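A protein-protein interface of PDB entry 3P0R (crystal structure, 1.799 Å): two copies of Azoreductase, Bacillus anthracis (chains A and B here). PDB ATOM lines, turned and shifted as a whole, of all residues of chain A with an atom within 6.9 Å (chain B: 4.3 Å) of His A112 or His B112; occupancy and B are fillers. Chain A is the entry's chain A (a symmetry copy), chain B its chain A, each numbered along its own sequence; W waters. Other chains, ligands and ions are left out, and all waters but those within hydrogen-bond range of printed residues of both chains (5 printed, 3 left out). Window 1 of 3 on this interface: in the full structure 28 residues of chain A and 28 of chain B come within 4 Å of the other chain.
Water W3 bridges O of Asp B116 and ND2 of Asn A104.
Water W2 lies within hydrogen-bond range of the side-chain carboxylate of Asp A116 (2.8 Å), a ring nitrogen (NE2) of His A112 (2.9 Å) and the backbone carbonyl oxygen of Ile B107 (3.5 Å).
Water W1 lies within hydrogen-bond range of N of Val B110 (3.0 Å), N of Ala B109 (3.1 Å) and O of Val A55 (3.2 Å).
Water W4 lies within hydrogen-bond range of the side-chain hydroxyl of Thr A106 (3.1 Å), a ring nitrogen (ND1) of His A112 (3.3 Å) and a ring nitrogen (ND1) of His B112 (3.4 Å).
Water W5 lies within hydrogen-bond range of OG1 of Thr B106 (3.1 Å), ND1 of His B112 (3.3 Å) and ND1 of His A112 (3.4 Å).
Thr A106 touches His B112, and with the chains exchanged His A112 touches Thr B106.
Ile A107 touches His B112, and with the chains exchanged His A112 touches Ile B107.
Pro A108 touches His B112, and with the chains exchanged His A112 touches Pro B108.
Ala A109 touches Thr B113, and with the chains exchanged Thr A113 touches Ala B109.
Of the 16 pairs that touch across the chains among the printed residues, 11 have their exchanged pair printed and touching as well.
Printed residues of chain A that touch a printed residue of chain B: Tyr A54, Asn A104, Thr A106, Ile A107, Pro A108, Ala A109, His A112, Thr A113 and Tyr A165.
Hydrophobic or aromatic side chains of chain A that line the printed part of chain B: Tyr A54, Ala A109, His A112 and Tyr A165.
Of the 11 printed residues of chain B, 8 touch a printed residue of chain A.
Hydrophobic or aromatic side chains of chain B within 4 Å of the printed part of chain A: Ala B109, Val B110 and His B112.
Among the printed residues, 16 pairs touch across the chains.
Among the printed residues, no Asp or Glu carboxylate lies within 4 Å of a Lys or Arg side-chain nitrogen of the other chain.
ND1 of His B112 is in hydrogen-bond range of ND1 of His A112 (3.0 Å).
OD1 of Asp B116 is in hydrogen-bond range of ND2 of Asn A104, at 2.9 Å.
The side-chain hydroxyl (OG1) of Thr B113 lies within hydrogen-bond range of the side-chain hydroxyl (OH) of Tyr A54 (2.8 Å).
NE2 of His A112 lies close to O of Ile B107, at 3.2 Å.
NE2 of His B112 lies close to O of Ile A107, at 3.2 Å.
C of Ala B109 touches CE1 of Tyr A54, 3.6 Å away.
CG1 of Val B110 touches CG of Tyr A54, 3.4 Å away.
His B112 touches Thr A106 (NE2 to CG2, 3.4 Å).
C of Pro A108 touches CE1 of His B112 (3.9 Å).
Ala A109 touches His B112 (N to CE1, 3.5 Å).
OG1 of Thr B113 touches CB of Ala A109, at 3.4 Å.
CG2 of Thr B106 touches NE2 of His A112, 3.4 Å away.
Pro B108 touches His A112.
His A112 touches Ala B109.
Tyr A165 touches Thr B106 (CE1 to CG2, 3.6 Å).
Of the printed residues of chain B, Pro A108 touches His B112.
Of the printed residues of chain B, Ala A109 touches His B112 and Thr B113.
Of chain B, only Thr B106, Ile B107, Pro B108, Ala B109 and His B112 come within 4 Å of His A112.
Of the printed residues of chain B, Thr A113 touches Ala B109 (3.4 Å).
His B112 touches just these residues of chain A: Thr A106, Ile A107, Pro A108, Ala A109 and His A112.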
ATOM      1  N   LEU A  47      -0.716  22.210  10.366  1.00  0.00           N
ATOM      2  CA  LEU A  47      -0.591  20.766  10.209  1.00  0.00           C
ATOM      3  C   LEU A  47      -0.478  20.062  11.549  1.00  0.00           C
ATOM      4  O   LEU A  47      -0.840  18.879  11.667  1.00  0.00           O
ATOM      5  CB  LEU A  47       0.551  20.409   9.283  1.00  0.00           C
ATOM      6  CG  LEU A  47       0.445  20.848   7.825  1.00  0.00           C
ATOM      7  CD1 LEU A  47       1.778  20.466   7.134  1.00  0.00           C
ATOM      8  CD2 LEU A  47      -0.825  20.245   7.165  1.00  0.00           C
ATOM      9  N   TYR A  54       0.097   8.382   8.045  1.00  0.00           N
ATOM     10  CA  TYR A  54       1.146   8.167   7.071  1.00  0.00           C
ATOM     11  C   TYR A  54       0.652   7.393   5.830  1.00  0.00           C
ATOM     12  O   TYR A  54      -0.219   6.496   5.905  1.00  0.00           O
ATOM     13  CB  TYR A  54       2.288   7.373   7.684  1.00  0.00           C
ATOM     14  CG  TYR A  54       3.064   8.053   8.795  1.00  0.00           C
ATOM     15  CD1 TYR A  54       4.084   8.951   8.483  1.00  0.00           C
ATOM     16  CD2 TYR A  54       2.808   7.800  10.121  1.00  0.00           C
ATOM     17  CE1 TYR A  54       4.801   9.602   9.481  1.00  0.00           C
ATOM     18  CE2 TYR A  54       3.548   8.428  11.122  1.00  0.00           C
ATOM     19  CZ  TYR A  54       4.539   9.328  10.794  1.00  0.00           C
ATOM     20  OH  TYR A  54       5.280   9.905  11.813  1.00  0.00           O
ATOM     21  N   VAL A  55       1.240   7.742   4.710  1.00  0.00           N
ATOM     22  CA  VAL A  55       1.054   7.013   3.462  1.00  0.00           C
ATOM     23  C   VAL A  55       1.767   5.665   3.452  1.00  0.00           C
ATOM     24  O   VAL A  55       3.015   5.570   3.577  1.00  0.00           O
ATOM     25  CB  VAL A  55       1.494   7.867   2.258  1.00  0.00           C
ATOM     26  CG1 VAL A  55       1.367   7.089   0.959  1.00  0.00           C
ATOM     27  CG2 VAL A  55       0.585   9.118   2.158  1.00  0.00           C
ATOM     28  N   TRP A 103      14.614  21.329   9.579  1.00  0.00           N
ATOM     29  CA  TRP A 103      14.984  20.501  10.715  1.00  0.00           C
ATOM     30  C   TRP A 103      15.585  19.215  10.185  1.00  0.00           C
ATOM     31  O   TRP A 103      14.975  18.543   9.357  1.00  0.00           O
ATOM     32  CB  TRP A 103      13.736  20.130  11.552  1.00  0.00           C
ATOM     33  CG  TRP A 103      13.011  21.242  12.274  1.00  0.00           C
ATOM     34  CD1 TRP A 103      13.482  22.478  12.614  1.00  0.00           C
ATOM     35  CD2 TRP A 103      11.721  21.134  12.883  1.00  0.00           C
ATOM     36  NE1 TRP A 103      12.543  23.148  13.348  1.00  0.00           N
ATOM     37  CE2 TRP A 103      11.443  22.360  13.500  1.00  0.00           C
ATOM     38  CE3 TRP A 103      10.756  20.141  12.907  1.00  0.00           C
ATOM     39  CZ2 TRP A 103      10.219  22.614  14.161  1.00  0.00           C
ATOM     40  CZ3 TRP A 103       9.550  20.391  13.590  1.00  0.00           C
ATOM     41  CH2 TRP A 103       9.311  21.617  14.201  1.00  0.00           C
ATOM     42  N   ASN A 104      16.767  18.853  10.655  1.00  0.00           N
ATOM     43  CA  ASN A 104      17.393  17.603  10.192  1.00  0.00           C
ATOM     44  C   ASN A 104      17.442  17.614   8.638  1.00  0.00           C
ATOM     45  O   ASN A 104      17.011  16.690   7.975  1.00  0.00           O
ATOM     46  CB  ASN A 104      16.667  16.362  10.765  1.00  0.00           C
ATOM     47  CG  ASN A 104      16.605  16.365  12.297  1.00  0.00           C
ATOM     48  OD1 ASN A 104      17.538  16.811  12.971  1.00  0.00           O
ATOM     49  ND2 ASN A 104      15.484  15.891  12.846  1.00  0.00           N
ATOM     50  N   THR A 106      15.727  18.942   6.326  1.00  0.00           N
ATOM     51  CA  THR A 106      14.540  18.882   5.513  1.00  0.00           C
ATOM     52  C   THR A 106      13.347  19.521   6.214  1.00  0.00           C
ATOM     53  O   THR A 106      13.477  20.179   7.257  1.00  0.00           O
ATOM     54  CB  THR A 106      14.263  17.402   5.099  1.00  0.00           C
ATOM     55  OG1 THR A 106      13.290  17.364   4.047  1.00  0.00           O
ATOM     56  CG2 THR A 106      13.843  16.529   6.274  1.00  0.00           C
ATOM     57  N   ILE A 107      12.193  19.330   5.608  1.00  0.00           N
ATOM     58  CA  ILE A 107      10.957  19.866   6.110  1.00  0.00           C
ATOM     59  C   ILE A 107      10.491  18.982   7.293  1.00  0.00           C
ATOM     60  O   ILE A 107      10.881  17.808   7.397  1.00  0.00           O
ATOM     61  CB  ILE A 107       9.879  19.936   4.988  1.00  0.00           C
ATOM     62  CG1 ILE A 107       9.660  18.567   4.347  1.00  0.00           C
ATOM     63  CG2 ILE A 107      10.188  21.120   3.980  1.00  0.00           C
ATOM     64  CD1 ILE A 107       8.418  18.561   3.274  1.00  0.00           C
ATOM     65  N   PRO A 108       9.632  19.526   8.181  1.00  0.00           N
ATOM     66  CA  PRO A 108       8.973  18.663   9.161  1.00  0.00           C
ATOM     67  C   PRO A 108       8.198  17.508   8.513  1.00  0.00           C
ATOM     68  O   PRO A 108       7.598  17.657   7.440  1.00  0.00           O
ATOM     69  CB  PRO A 108       8.009  19.632   9.862  1.00  0.00           C
ATOM     70  CG  PRO A 108       8.784  20.919   9.846  1.00  0.00           C
ATOM     71  CD  PRO A 108       9.305  20.949   8.430  1.00  0.00           C
ATOM     72  N   ALA A 109       8.301  16.347   9.109  1.00  0.00           N
ATOM     73  CA  ALA A 109       7.613  15.168   8.591  1.00  0.00           C
ATOM     74  C   ALA A 109       6.101  15.367   8.395  1.00  0.00           C
ATOM     75  O   ALA A 109       5.522  14.808   7.430  1.00  0.00           O
ATOM     76  CB  ALA A 109       7.886  13.923   9.451  1.00  0.00           C
ATOM     77  N   VAL A 110       5.463  16.214   9.201  1.00  0.00           N
ATOM     78  CA  VAL A 110       4.041  16.576   8.949  1.00  0.00           C
ATOM     79  C   VAL A 110       3.803  17.172   7.570  1.00  0.00           C
ATOM     80  O   VAL A 110       2.820  16.850   6.874  1.00  0.00           O
ATOM     81  CB  VAL A 110       3.458  17.578  10.039  1.00  0.00           C
ATOM     82  CG1 VAL A 110       3.320  16.889  11.398  1.00  0.00           C
ATOM     83  CG2 VAL A 110       4.240  18.887  10.101  1.00  0.00           C
ATOM     84  N   LEU A 111       4.723  18.028   7.136  1.00  0.00           N
ATOM     85  CA  LEU A 111       4.623  18.612   5.795  1.00  0.00           C
ATOM     86  C   LEU A 111       5.001  17.599   4.724  1.00  0.00           C
ATOM     87  O   LEU A 111       4.471  17.636   3.643  1.00  0.00           O
ATOM     88  CB  LEU A 111       5.506  19.845   5.643  1.00  0.00           C
ATOM     89  CG  LEU A 111       5.401  20.621   4.321  1.00  0.00           C
ATOM     90  CD1 LEU A 111       3.939  21.027   3.978  1.00  0.00           C
ATOM     91  CD2 LEU A 111       6.330  21.871   4.407  1.00  0.00           C
ATOM     92  N   HIS A 112       5.896  16.683   5.038  1.00  0.00           N
ATOM     93  CA  HIS A 112       6.233  15.628   4.123  1.00  0.00           C
ATOM     94  C   HIS A 112       4.961  14.773   3.804  1.00  0.00           C
ATOM     95  O   HIS A 112       4.616  14.535   2.642  1.00  0.00           O
ATOM     96  CB  HIS A 112       7.344  14.818   4.759  1.00  0.00           C
ATOM     97  CG  HIS A 112       7.778  13.641   3.984  1.00  0.00           C
ATOM     98  ND1 HIS A 112       8.859  12.887   4.387  1.00  0.00           N
ATOM     99  CD2 HIS A 112       7.312  13.065   2.845  1.00  0.00           C
ATOM    100  CE1 HIS A 112       9.030  11.896   3.532  1.00  0.00           C
ATOM    101  NE2 HIS A 112       8.092  11.957   2.610  1.00  0.00           N
ATOM    102  N   THR A 113       4.237  14.381   4.844  1.00  0.00           N
ATOM    103  CA  THR A 113       2.971  13.621   4.688  1.00  0.00           C
ATOM    104  C   THR A 113       1.920  14.433   3.933  1.00  0.00           C
ATOM    105  O   THR A 113       1.260  13.921   3.008  1.00  0.00           O
ATOM    106  CB  THR A 113       2.435  13.145   6.051  1.00  0.00           C
ATOM    107  OG1 THR A 113       3.284  12.106   6.578  1.00  0.00           O
ATOM    108  CG2 THR A 113       0.967  12.652   5.902  1.00  0.00           C
ATOM    109  N   TYR A 114       1.776  15.705   4.259  1.00  0.00           N
ATOM    110  CA  TYR A 114       0.860  16.590   3.521  1.00  0.00           C
ATOM    111  C   TYR A 114       1.161  16.581   2.009  1.00  0.00           C
ATOM    112  O   TYR A 114       0.231  16.449   1.173  1.00  0.00           O
ATOM    113  CB  TYR A 114       0.863  17.996   4.129  1.00  0.00           C
ATOM    114  CG  TYR A 114      -0.030  18.985   3.440  1.00  0.00           C
ATOM    115  CD1 TYR A 114      -1.407  19.005   3.674  1.00  0.00           C
ATOM    116  CD2 TYR A 114       0.493  19.894   2.549  1.00  0.00           C
ATOM    117  CE1 TYR A 114      -2.238  19.924   3.003  1.00  0.00           C
ATOM    118  CE2 TYR A 114      -0.327  20.815   1.874  1.00  0.00           C
ATOM    119  CZ  TYR A 114      -1.681  20.828   2.115  1.00  0.00           C
ATOM    120  OH  TYR A 114      -2.513  21.751   1.452  1.00  0.00           O
ATOM    121  N   ILE A 115       2.433  16.703   1.653  1.00  0.00           N
ATOM    122  CA  ILE A 115       2.827  16.748   0.257  1.00  0.00           C
ATOM    123  C   ILE A 115       2.573  15.407  -0.392  1.00  0.00           C
ATOM    124  O   ILE A 115       2.110  15.325  -1.555  1.00  0.00           O
ATOM    125  CB  ILE A 115       4.268  17.289   0.055  1.00  0.00           C
ATOM    126  CG1 ILE A 115       4.349  18.792   0.451  1.00  0.00           C
ATOM    127  CG2 ILE A 115       4.702  17.038  -1.447  1.00  0.00           C
ATOM    128  CD1 ILE A 115       5.794  19.358   0.595  1.00  0.00           C
ATOM    129  N   ASP A 116       2.844  14.331   0.344  1.00  0.00           N
ATOM    130  CA  ASP A 116       2.506  12.991  -0.142  1.00  0.00           C
ATOM    131  C   ASP A 116       1.039  12.909  -0.554  1.00  0.00           C
ATOM    132  O   ASP A 116       0.716  12.325  -1.617  1.00  0.00           O
ATOM    133  CB  ASP A 116       2.737  11.899   0.910  1.00  0.00           C
ATOM    134  CG  ASP A 116       4.195  11.627   1.193  1.00  0.00           C
ATOM    135  OD1 ASP A 116       5.051  11.871   0.309  1.00  0.00           O
ATOM    136  OD2 ASP A 116       4.478  11.077   2.306  1.00  0.00           O
ATOM    137  N   TYR A 117       0.154  13.501   0.243  1.00  0.00           N
ATOM    138  CA  TYR A 117      -1.268  13.511  -0.083  1.00  0.00           C
ATOM    139  C   TYR A 117      -1.559  14.239  -1.408  1.00  0.00           C
ATOM    140  O   TYR A 117      -2.497  13.850  -2.122  1.00  0.00           O
ATOM    141  CB  TYR A 117      -2.094  14.167   1.026  1.00  0.00           C
ATOM    142  CG  TYR A 117      -2.092  13.544   2.401  1.00  0.00           C
ATOM    143  CD1 TYR A 117      -1.743  12.215   2.622  1.00  0.00           C
ATOM    144  CD2 TYR A 117      -2.553  14.287   3.475  1.00  0.00           C
ATOM    145  CE1 TYR A 117      -1.808  11.650   3.915  1.00  0.00           C
ATOM    146  CE2 TYR A 117      -2.654  13.768   4.725  1.00  0.00           C
ATOM    147  CZ  TYR A 117      -2.263  12.457   4.974  1.00  0.00           C
ATOM    148  OH  TYR A 117      -2.342  11.972   6.258  1.00  0.00           O
ATOM    149  N   TYR A 165      13.164  20.347  -1.489  1.00  0.00           N
ATOM    150  CA  TYR A 165      12.145  19.322  -1.523  1.00  0.00           C
ATOM    151  C   TYR A 165      10.801  19.898  -1.984  1.00  0.00           C
ATOM    152  O   TYR A 165      10.171  19.435  -2.971  1.00  0.00           O
ATOM    153  CB  TYR A 165      11.989  18.585  -0.158  1.00  0.00           C
ATOM    154  CG  TYR A 165      10.999  17.458  -0.366  1.00  0.00           C
ATOM    155  CD1 TYR A 165      11.394  16.304  -1.012  1.00  0.00           C
ATOM    156  CD2 TYR A 165       9.646  17.584  -0.001  1.00  0.00           C
ATOM    157  CE1 TYR A 165      10.510  15.288  -1.272  1.00  0.00           C
ATOM    158  CE2 TYR A 165       8.730  16.574  -0.266  1.00  0.00           C
ATOM    159  CZ  TYR A 165       9.171  15.401  -0.900  1.00  0.00           C
ATOM    160  OH  TYR A 165       8.288  14.387  -1.207  1.00  0.00           O
ATOM    161  N   THR B 106      11.906  10.955  -2.089  1.00  0.00           N
ATOM    162  CA  THR B 106      12.507  10.785  -0.792  1.00  0.00           C
ATOM    163  C   THR B 106      12.044   9.496  -0.123  1.00  0.00           C
ATOM    164  O   THR B 106      11.399   8.635  -0.740  1.00  0.00           O
ATOM    165  CB  THR B 106      12.223  12.044   0.087  1.00  0.00           C
ATOM    166  OG1 THR B 106      13.067  12.032   1.245  1.00  0.00           O
ATOM    167  CG2 THR B 106      10.755  12.176   0.472  1.00  0.00           C
ATOM    168  N   ILE B 107      12.406   9.375   1.138  1.00  0.00           N
ATOM    169  CA  ILE B 107      12.075   8.224   1.931  1.00  0.00           C
ATOM    170  C   ILE B 107      10.591   8.342   2.360  1.00  0.00           C
ATOM    171  O   ILE B 107      10.030   9.449   2.398  1.00  0.00           O
ATOM    172  CB  ILE B 107      13.019   8.102   3.164  1.00  0.00           C
ATOM    173  CG1 ILE B 107      12.991   9.374   4.009  1.00  0.00           C
ATOM    174  CG2 ILE B 107      14.459   7.605   2.726  1.00  0.00           C
ATOM    175  CD1 ILE B 107      13.844   9.227   5.404  1.00  0.00           C
ATOM    176  N   PRO B 108       9.949   7.209   2.714  1.00  0.00           N
ATOM    177  CA  PRO B 108       8.640   7.299   3.361  1.00  0.00           C
ATOM    178  C   PRO B 108       8.661   8.158   4.632  1.00  0.00           C
ATOM    179  O   PRO B 108       9.638   8.157   5.394  1.00  0.00           O
ATOM    180  CB  PRO B 108       8.338   5.833   3.706  1.00  0.00           C
ATOM    181  CG  PRO B 108       8.971   5.099   2.558  1.00  0.00           C
ATOM    182  CD  PRO B 108      10.304   5.797   2.441  1.00  0.00           C
ATOM    183  N   ALA B 109       7.638   8.958   4.797  1.00  0.00           N
ATOM    184  CA  ALA B 109       7.539   9.828   5.966  1.00  0.00           C
ATOM    185  C   ALA B 109       7.668   9.086   7.306  1.00  0.00           C
ATOM    186  O   ALA B 109       8.246   9.644   8.272  1.00  0.00           O
ATOM    187  CB  ALA B 109       6.258  10.676   5.940  1.00  0.00           C
ATOM    188  N   VAL B 110       7.248   7.823   7.374  1.00  0.00           N
ATOM    189  CA  VAL B 110       7.504   7.004   8.590  1.00  0.00           C
ATOM    190  C   VAL B 110       8.979   6.893   8.947  1.00  0.00           C
ATOM    191  O   VAL B 110       9.380   6.986  10.123  1.00  0.00           O
ATOM    192  CB  VAL B 110       6.900   5.535   8.482  1.00  0.00           C
ATOM    193  CG1 VAL B 110       5.371   5.569   8.501  1.00  0.00           C
ATOM    194  CG2 VAL B 110       7.472   4.758   7.299  1.00  0.00           C
ATOM    195  N   LEU B 111       9.815   6.727   7.928  1.00  0.00           N
ATOM    196  CA  LEU B 111      11.263   6.672   8.155  1.00  0.00           C
ATOM    197  C   LEU B 111      11.827   8.055   8.447  1.00  0.00           C
ATOM    198  O   LEU B 111      12.769   8.180   9.187  1.00  0.00           O
ATOM    199  CB  LEU B 111      12.005   6.077   6.963  1.00  0.00           C
ATOM    200  CG  LEU B 111      13.517   5.853   7.122  1.00  0.00           C
ATOM    201  CD1 LEU B 111      13.870   5.012   8.382  1.00  0.00           C
ATOM    202  CD2 LEU B 111      14.055   5.180   5.822  1.00  0.00           C
ATOM    203  N   HIS B 112      11.232   9.089   7.885  1.00  0.00           N
ATOM    204  CA  HIS B 112      11.634  10.434   8.189  1.00  0.00           C
ATOM    205  C   HIS B 112      11.444  10.715   9.717  1.00  0.00           C
ATOM    206  O   HIS B 112      12.357  11.176  10.410  1.00  0.00           O
ATOM    207  CB  HIS B 112      10.814  11.358   7.313  1.00  0.00           C
ATOM    208  CG  HIS B 112      11.047  12.797   7.536  1.00  0.00           C
ATOM    209  ND1 HIS B 112      10.457  13.744   6.727  1.00  0.00           N
ATOM    210  CD2 HIS B 112      11.784  13.480   8.451  1.00  0.00           C
ATOM    211  CE1 HIS B 112      10.818  14.944   7.141  1.00  0.00           C
ATOM    212  NE2 HIS B 112      11.591  14.818   8.200  1.00  0.00           N
ATOM    213  N   THR B 113      10.277  10.364  10.241  1.00  0.00           N
ATOM    214  CA  THR B 113       9.981  10.511  11.688  1.00  0.00           C
ATOM    215  C   THR B 113      10.914   9.653  12.540  1.00  0.00           C
ATOM    216  O   THR B 113      11.469  10.123  13.552  1.00  0.00           O
ATOM    217  CB  THR B 113       8.504  10.196  11.989  1.00  0.00           C
ATOM    218  OG1 THR B 113       7.660  11.237  11.458  1.00  0.00           O
ATOM    219  CG2 THR B 113       8.297  10.032  13.523  1.00  0.00           C
ATOM    220  N   TYR B 114      11.152   8.417  12.137  1.00  0.00           N
ATOM    221  CA  TYR B 114      12.113   7.551  12.837  1.00  0.00           C
ATOM    222  C   TYR B 114      13.497   8.220  12.956  1.00  0.00           C
ATOM    223  O   TYR B 114      14.111   8.228  14.054  1.00  0.00           O
ATOM    224  CB  TYR B 114      12.167   6.167  12.182  1.00  0.00           C
ATOM    225  CG  TYR B 114      13.132   5.205  12.812  1.00  0.00           C
ATOM    226  CD1 TYR B 114      12.808   4.518  13.984  1.00  0.00           C
ATOM    227  CD2 TYR B 114      14.367   4.988  12.248  1.00  0.00           C
ATOM    228  CE1 TYR B 114      13.731   3.634  14.579  1.00  0.00           C
ATOM    229  CE2 TYR B 114      15.296   4.109  12.834  1.00  0.00           C
ATOM    230  CZ  TYR B 114      14.966   3.434  13.986  1.00  0.00           C
ATOM    231  OH  TYR B 114      15.883   2.545  14.578  1.00  0.00           O
ATOM    232  N   ILE B 115      13.981   8.788  11.860  1.00  0.00           N
ATOM    233  CA  ILE B 115      15.291   9.413  11.847  1.00  0.00           C
ATOM    234  C   ILE B 115      15.280  10.649  12.716  1.00  0.00           C
ATOM    235  O   ILE B 115      16.250  10.930  13.459  1.00  0.00           O
ATOM    236  CB  ILE B 115      15.831   9.650  10.411  1.00  0.00           C
ATOM    237  CG1 ILE B 115      16.124   8.294   9.706  1.00  0.00           C
ATOM    238  CG2 ILE B 115      17.114  10.575  10.494  1.00  0.00           C
ATOM    239  CD1 ILE B 115      16.364   8.389   8.168  1.00  0.00           C
ATOM    240  N   ASP B 116      14.181  11.400  12.664  1.00  0.00           N
ATOM    241  CA  ASP B 116      14.017  12.543  13.565  1.00  0.00           C
ATOM    242  C   ASP B 116      14.223  12.130  15.020  1.00  0.00           C
ATOM    243  O   ASP B 116      14.901  12.853  15.789  1.00  0.00           O
ATOM    244  CB  ASP B 116      12.624  13.178  13.475  1.00  0.00           C
ATOM    245  CG  ASP B 116      12.381  13.928  12.186  1.00  0.00           C
ATOM    246  OD1 ASP B 116      13.356  14.403  11.556  1.00  0.00           O
ATOM    247  OD2 ASP B 116      11.170  14.113  11.840  1.00  0.00           O
HETATM  248  O   HOH W   1       5.068   7.254   5.337  1.00  0.00           O
HETATM  249  O   HOH W   2       7.399  10.281   0.315  1.00  0.00           O
HETATM  250  O   HOH W   3      14.816  15.665  15.724  1.00  0.00           O
HETATM  251  O   HOH W   4      10.882  15.497   3.828  1.00  0.00           O
HETATM  252  O   HOH W   5      12.254  12.634   4.128  1.00  0.00           O
